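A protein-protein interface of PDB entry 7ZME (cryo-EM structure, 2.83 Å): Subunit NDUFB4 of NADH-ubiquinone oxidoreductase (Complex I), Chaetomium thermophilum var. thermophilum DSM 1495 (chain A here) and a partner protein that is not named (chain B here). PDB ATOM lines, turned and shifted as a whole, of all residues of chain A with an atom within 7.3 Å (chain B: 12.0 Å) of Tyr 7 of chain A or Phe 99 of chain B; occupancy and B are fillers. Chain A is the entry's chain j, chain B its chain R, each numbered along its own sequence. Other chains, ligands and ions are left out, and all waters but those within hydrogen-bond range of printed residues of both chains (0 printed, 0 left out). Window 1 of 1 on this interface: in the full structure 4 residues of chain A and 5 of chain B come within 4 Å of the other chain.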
ATOM      1  N   LEU A   4     -16.509 -12.741  -4.191  1.00  0.00           N
ATOM      2  CA  LEU A   4     -15.524 -13.805  -4.303  1.00  0.00           C
ATOM      3  C   LEU A   4     -14.452 -13.661  -3.229  1.00  0.00           C
ATOM      4  O   LEU A   4     -14.070 -12.553  -2.842  1.00  0.00           O
ATOM      5  CB  LEU A   4     -14.898 -13.805  -5.701  1.00  0.00           C
ATOM      6  CG  LEU A   4     -14.169 -12.562  -6.222  1.00  0.00           C
ATOM      7  CD1 LEU A   4     -12.705 -12.516  -5.794  1.00  0.00           C
ATOM      8  CD2 LEU A   4     -14.286 -12.477  -7.739  1.00  0.00           C
ATOM      9  N   GLN A   5     -13.976 -14.800  -2.737  1.00  0.00           N
ATOM     10  CA  GLN A   5     -12.978 -14.793  -1.681  1.00  0.00           C
ATOM     11  C   GLN A   5     -11.659 -14.232  -2.192  1.00  0.00           C
ATOM     12  O   GLN A   5     -11.315 -14.359  -3.370  1.00  0.00           O
ATOM     13  CB  GLN A   5     -12.775 -16.201  -1.122  1.00  0.00           C
ATOM     14  CG  GLN A   5     -12.188 -17.192  -2.109  1.00  0.00           C
ATOM     15  CD  GLN A   5     -12.068 -18.585  -1.526  1.00  0.00           C
ATOM     16  OE1 GLN A   5     -12.377 -18.808  -0.356  1.00  0.00           O
ATOM     17  NE2 GLN A   5     -11.617 -19.532  -2.340  1.00  0.00           N
ATOM     18  N   HIS A   6     -10.921 -13.599  -1.288  1.00  0.00           N
ATOM     19  CA  HIS A   6      -9.649 -12.968  -1.591  1.00  0.00           C
ATOM     20  C   HIS A   6      -8.519 -13.745  -0.925  1.00  0.00           C
ATOM     21  O   HIS A   6      -8.727 -14.795  -0.314  1.00  0.00           O
ATOM     22  CB  HIS A   6      -9.663 -11.505  -1.150  1.00  0.00           C
ATOM     23  CG  HIS A   6     -10.009 -11.310   0.292  1.00  0.00           C
ATOM     24  ND1 HIS A   6      -9.059 -11.288   1.289  1.00  0.00           N
ATOM     25  CD2 HIS A   6     -11.202 -11.123   0.905  1.00  0.00           C
ATOM     26  CE1 HIS A   6      -9.650 -11.099   2.454  1.00  0.00           C
ATOM     27  NE2 HIS A   6     -10.951 -10.997   2.249  1.00  0.00           N
ATOM     28  N   TYR A   7      -7.305 -13.219  -1.057  1.00  0.00           N
ATOM     29  CA  TYR A   7      -6.151 -13.852  -0.443  1.00  0.00           C
ATOM     30  C   TYR A   7      -6.164 -13.629   1.062  1.00  0.00           C
ATOM     31  O   TYR A   7      -6.851 -12.745   1.580  1.00  0.00           O
ATOM     32  CB  TYR A   7      -4.856 -13.307  -1.041  1.00  0.00           C
ATOM     33  CG  TYR A   7      -4.523 -13.881  -2.393  1.00  0.00           C
ATOM     34  CD1 TYR A   7      -4.328 -15.240  -2.556  1.00  0.00           C
ATOM     35  CD2 TYR A   7      -4.409 -13.065  -3.506  1.00  0.00           C
ATOM     36  CE1 TYR A   7      -4.030 -15.771  -3.789  1.00  0.00           C
ATOM     37  CE2 TYR A   7      -4.103 -13.585  -4.743  1.00  0.00           C
ATOM     38  CZ  TYR A   7      -3.918 -14.942  -4.879  1.00  0.00           C
ATOM     39  OH  TYR A   7      -3.617 -15.480  -6.106  1.00  0.00           O
ATOM     40  N   LYS A   8      -5.392 -14.447   1.770  1.00  0.00           N
ATOM     41  CA  LYS A   8      -5.310 -14.343   3.220  1.00  0.00           C
ATOM     42  C   LYS A   8      -4.401 -13.180   3.596  1.00  0.00           C
ATOM     43  O   LYS A   8      -3.240 -13.128   3.178  1.00  0.00           O
ATOM     44  CB  LYS A   8      -4.809 -15.652   3.826  1.00  0.00           C
ATOM     45  CG  LYS A   8      -5.754 -16.827   3.605  1.00  0.00           C
ATOM     46  CD  LYS A   8      -5.253 -18.091   4.286  1.00  0.00           C
ATOM     47  CE  LYS A   8      -4.024 -18.655   3.594  1.00  0.00           C
ATOM     48  NZ  LYS A   8      -4.336 -19.137   2.221  1.00  0.00           N
ATOM     49  N   ILE A   9      -4.935 -12.249   4.380  1.00  0.00           N
ATOM     50  CA  ILE A   9      -4.251 -11.018   4.752  1.00  0.00           C
ATOM     51  C   ILE A   9      -4.072 -11.011   6.261  1.00  0.00           C
ATOM     52  O   ILE A   9      -5.022 -11.281   7.003  1.00  0.00           O
ATOM     53  CB  ILE A   9      -5.036  -9.776   4.288  1.00  0.00           C
ATOM     54  CG1 ILE A   9      -5.176  -9.771   2.765  1.00  0.00           C
ATOM     55  CG2 ILE A   9      -4.373  -8.488   4.779  1.00  0.00           C
ATOM     56  CD1 ILE A   9      -3.871  -9.642   2.035  1.00  0.00           C
ATOM     57  N   ALA A  10      -2.856 -10.704   6.712  1.00  0.00           N
ATOM     58  CA  ALA A  10      -2.562 -10.555   8.137  1.00  0.00           C
ATOM     59  C   ALA A  10      -3.155  -9.235   8.612  1.00  0.00           C
ATOM     60  O   ALA A  10      -2.478  -8.212   8.734  1.00  0.00           O
ATOM     61  CB  ALA A  10      -1.061 -10.608   8.388  1.00  0.00           C
ATOM     62  N   ASN B  90       7.867 -14.079   0.718  1.00  0.00           N
ATOM     63  CA  ASN B  90       7.075 -15.283   0.488  1.00  0.00           C
ATOM     64  C   ASN B  90       7.500 -15.907  -0.834  1.00  0.00           C
ATOM     65  O   ASN B  90       7.143 -15.407  -1.904  1.00  0.00           O
ATOM     66  CB  ASN B  90       5.587 -14.938   0.478  1.00  0.00           C
ATOM     67  CG  ASN B  90       4.703 -16.147   0.660  1.00  0.00           C
ATOM     68  OD1 ASN B  90       5.107 -17.275   0.392  1.00  0.00           O
ATOM     69  ND2 ASN B  90       3.484 -15.917   1.125  1.00  0.00           N
ATOM     70  N   GLU B  92       6.672 -18.989  -1.788  1.00  0.00           N
ATOM     71  CA  GLU B  92       5.690 -19.963  -2.227  1.00  0.00           C
ATOM     72  C   GLU B  92       4.755 -19.367  -3.276  1.00  0.00           C
ATOM     73  O   GLU B  92       4.451 -18.172  -3.240  1.00  0.00           O
ATOM     74  CB  GLU B  92       4.877 -20.467  -1.042  1.00  0.00           C
ATOM     75  CG  GLU B  92       5.523 -21.620  -0.288  1.00  0.00           C
ATOM     76  CD  GLU B  92       6.646 -21.172   0.628  1.00  0.00           C
ATOM     77  OE1 GLU B  92       6.922 -19.955   0.692  1.00  0.00           O
ATOM     78  OE2 GLU B  92       7.253 -22.042   1.287  1.00  0.00           O
ATOM     79  N   PRO B  93       4.292 -20.183  -4.217  1.00  0.00           N
ATOM     80  CA  PRO B  93       3.373 -19.694  -5.248  1.00  0.00           C
ATOM     81  C   PRO B  93       2.021 -19.343  -4.658  1.00  0.00           C
ATOM     82  O   PRO B  93       1.652 -19.836  -3.583  1.00  0.00           O
ATOM     83  CB  PRO B  93       3.263 -20.881  -6.216  1.00  0.00           C
ATOM     84  CG  PRO B  93       4.438 -21.744  -5.915  1.00  0.00           C
ATOM     85  CD  PRO B  93       4.707 -21.573  -4.459  1.00  0.00           C
ATOM     86  N   PRO B  94       1.259 -18.480  -5.328  1.00  0.00           N
ATOM     87  CA  PRO B  94      -0.068 -18.144  -4.832  1.00  0.00           C
ATOM     88  C   PRO B  94      -0.966 -19.365  -4.811  1.00  0.00           C
ATOM     89  O   PRO B  94      -0.874 -20.243  -5.687  1.00  0.00           O
ATOM     90  CB  PRO B  94      -0.569 -17.098  -5.839  1.00  0.00           C
ATOM     91  CG  PRO B  94       0.379 -17.147  -6.982  1.00  0.00           C
ATOM     92  CD  PRO B  94       1.672 -17.597  -6.427  1.00  0.00           C
ATOM     93  N   PRO B  95      -1.859 -19.454  -3.833  1.00  0.00           N
ATOM     94  CA  PRO B  95      -2.856 -20.521  -3.825  1.00  0.00           C
ATOM     95  C   PRO B  95      -3.835 -20.340  -4.967  1.00  0.00           C
ATOM     96  O   PRO B  95      -4.028 -19.219  -5.457  1.00  0.00           O
ATOM     97  CB  PRO B  95      -3.546 -20.340  -2.467  1.00  0.00           C
ATOM     98  CG  PRO B  95      -3.392 -18.892  -2.182  1.00  0.00           C
ATOM     99  CD  PRO B  95      -2.043 -18.520  -2.711  1.00  0.00           C
ATOM    100  N   PRO B  96      -4.479 -21.409  -5.420  1.00  0.00           N
ATOM    101  CA  PRO B  96      -5.362 -21.279  -6.584  1.00  0.00           C
ATOM    102  C   PRO B  96      -6.620 -20.492  -6.267  1.00  0.00           C
ATOM    103  O   PRO B  96      -7.548 -21.005  -5.635  1.00  0.00           O
ATOM    104  CB  PRO B  96      -5.685 -22.736  -6.941  1.00  0.00           C
ATOM    105  CG  PRO B  96      -5.498 -23.489  -5.669  1.00  0.00           C
ATOM    106  CD  PRO B  96      -4.387 -22.798  -4.938  1.00  0.00           C
ATOM    107  N   LEU B  97      -6.659 -19.243  -6.723  1.00  0.00           N
ATOM    108  CA  LEU B  97      -7.809 -18.365  -6.573  1.00  0.00           C
ATOM    109  C   LEU B  97      -8.127 -17.735  -7.918  1.00  0.00           C
ATOM    110  O   LEU B  97      -7.222 -17.446  -8.706  1.00  0.00           O
ATOM    111  CB  LEU B  97      -7.560 -17.259  -5.542  1.00  0.00           C
ATOM    112  CG  LEU B  97      -8.067 -17.415  -4.109  1.00  0.00           C
ATOM    113  CD1 LEU B  97      -7.602 -18.716  -3.481  1.00  0.00           C
ATOM    114  CD2 LEU B  97      -7.635 -16.230  -3.271  1.00  0.00           C
ATOM    115  N   LYS B  98      -9.409 -17.479  -8.171  1.00  0.00           N
ATOM    116  CA  LYS B  98      -9.774 -16.794  -9.438  1.00  0.00           C
ATOM    117  C   LYS B  98     -10.117 -15.330  -9.155  1.00  0.00           C
ATOM    118  O   LYS B  98     -10.915 -15.083  -8.232  1.00  0.00           O
ATOM    119  CB  LYS B  98     -10.946 -17.507 -10.121  1.00  0.00           C
ATOM    120  CG  LYS B  98     -10.568 -18.637 -11.069  1.00  0.00           C
ATOM    121  CD  LYS B  98     -10.094 -19.895 -10.373  1.00  0.00           C
ATOM    122  CE  LYS B  98      -9.721 -21.001 -11.337  1.00  0.00           C
ATOM    123  NZ  LYS B  98      -9.307 -22.233 -10.626  1.00  0.00           N
ATOM    124  N   PHE B  99      -9.492 -14.405  -9.885  1.00  0.00           N
ATOM    125  CA  PHE B  99      -9.877 -12.975  -9.762  1.00  0.00           C
ATOM    126  C   PHE B  99     -10.222 -12.466 -11.166  1.00  0.00           C
ATOM    127  O   PHE B  99     -11.384 -12.066 -11.349  1.00  0.00           O
ATOM    128  CB  PHE B  99      -8.756 -12.160  -9.114  1.00  0.00           C
ATOM    129  CG  PHE B  99      -8.376 -12.638  -7.741  1.00  0.00           C
ATOM    130  CD1 PHE B  99      -9.162 -12.329  -6.646  1.00  0.00           C
ATOM    131  CD2 PHE B  99      -7.247 -13.409  -7.549  1.00  0.00           C
ATOM    132  CE1 PHE B  99      -8.823 -12.780  -5.384  1.00  0.00           C
ATOM    133  CE2 PHE B  99      -6.914 -13.857  -6.284  1.00  0.00           C
ATOM    134  CZ  PHE B  99      -7.692 -13.529  -5.204  1.00  0.00           C
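Leu 4 of chain A touches Lys 98 of chain B (CD1 to O, 3.97 Å).
CD1 of Phe 99 of chain B touches CD1 of Leu 4 of chain A, at 3.6 Å.
CE1 of Phe 99 of chain B touches O of Gln 5 of chain A, 3.6 Å away.
Leu 97 of chain B touches His 6 of chain A.
Phe 99 of chain B touches His 6 of chain A.
OH of Tyr 7 of chain A touches CB of Pro 94 of chain B (3.5 Å).
CD of Pro 95 of chain B touches CE1 of Tyr 7 of chain A, at 3.6 Å.
CD2 of Leu 97 of chain B touches CD1 of Tyr 7 of chain A, at 3.5 Å.
Tyr 7 of chain A touches Phe 99 of chain B.
Printed residues of chain B that touch a printed residue of chain A: Pro 94, Pro 95, Leu 97, Lys 98 and Phe 99.
Of the 7 printed residues of chain A, 4 touch a printed residue of chain B.
Printed residues of chain A that touch a printed residue of chain B: Leu 4, Gln 5, His 6 and Tyr 7.
Hydrophobic or aromatic side chains of chain A that line the printed part of chain B: Leu 4 and Tyr 7.
Among the printed residues, no Asp or Glu carboxylate lies within 4 Å of a Lys or Arg side-chain nitrogen of the other chain.
Of chain B, only Lys 98 and Phe 99 come within 4 Å of Leu 4 of chain A.
Gln 5 of chain A touches one residue of chain B.
Of chain B, only Leu 97 (3.5 Å) and Phe 99 (3.9 Å) come within 4 Å of His 6 of chain A.
Printed residues of chain B within 4 Å of Tyr 7 of chain A: Pro 94, Pro 95, Leu 97 and Phe 99.
No residue of chain B comes within 4 Å of Ile 9 of chain A.
Of the printed residues of chain A, Pro 94 of chain B touches Tyr 7.
Of the printed residues of chain A, Pro 95 of chain B touches Tyr 7 (3.6 Å).
Of the printed residues of chain A, Leu 97 of chain B touches His 6 and Tyr 7.
Printed residues of chain A within 4 Å of Lys 98 of chain B: Leu 4.
Phe 99 of chain B touches four residues of chain A.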
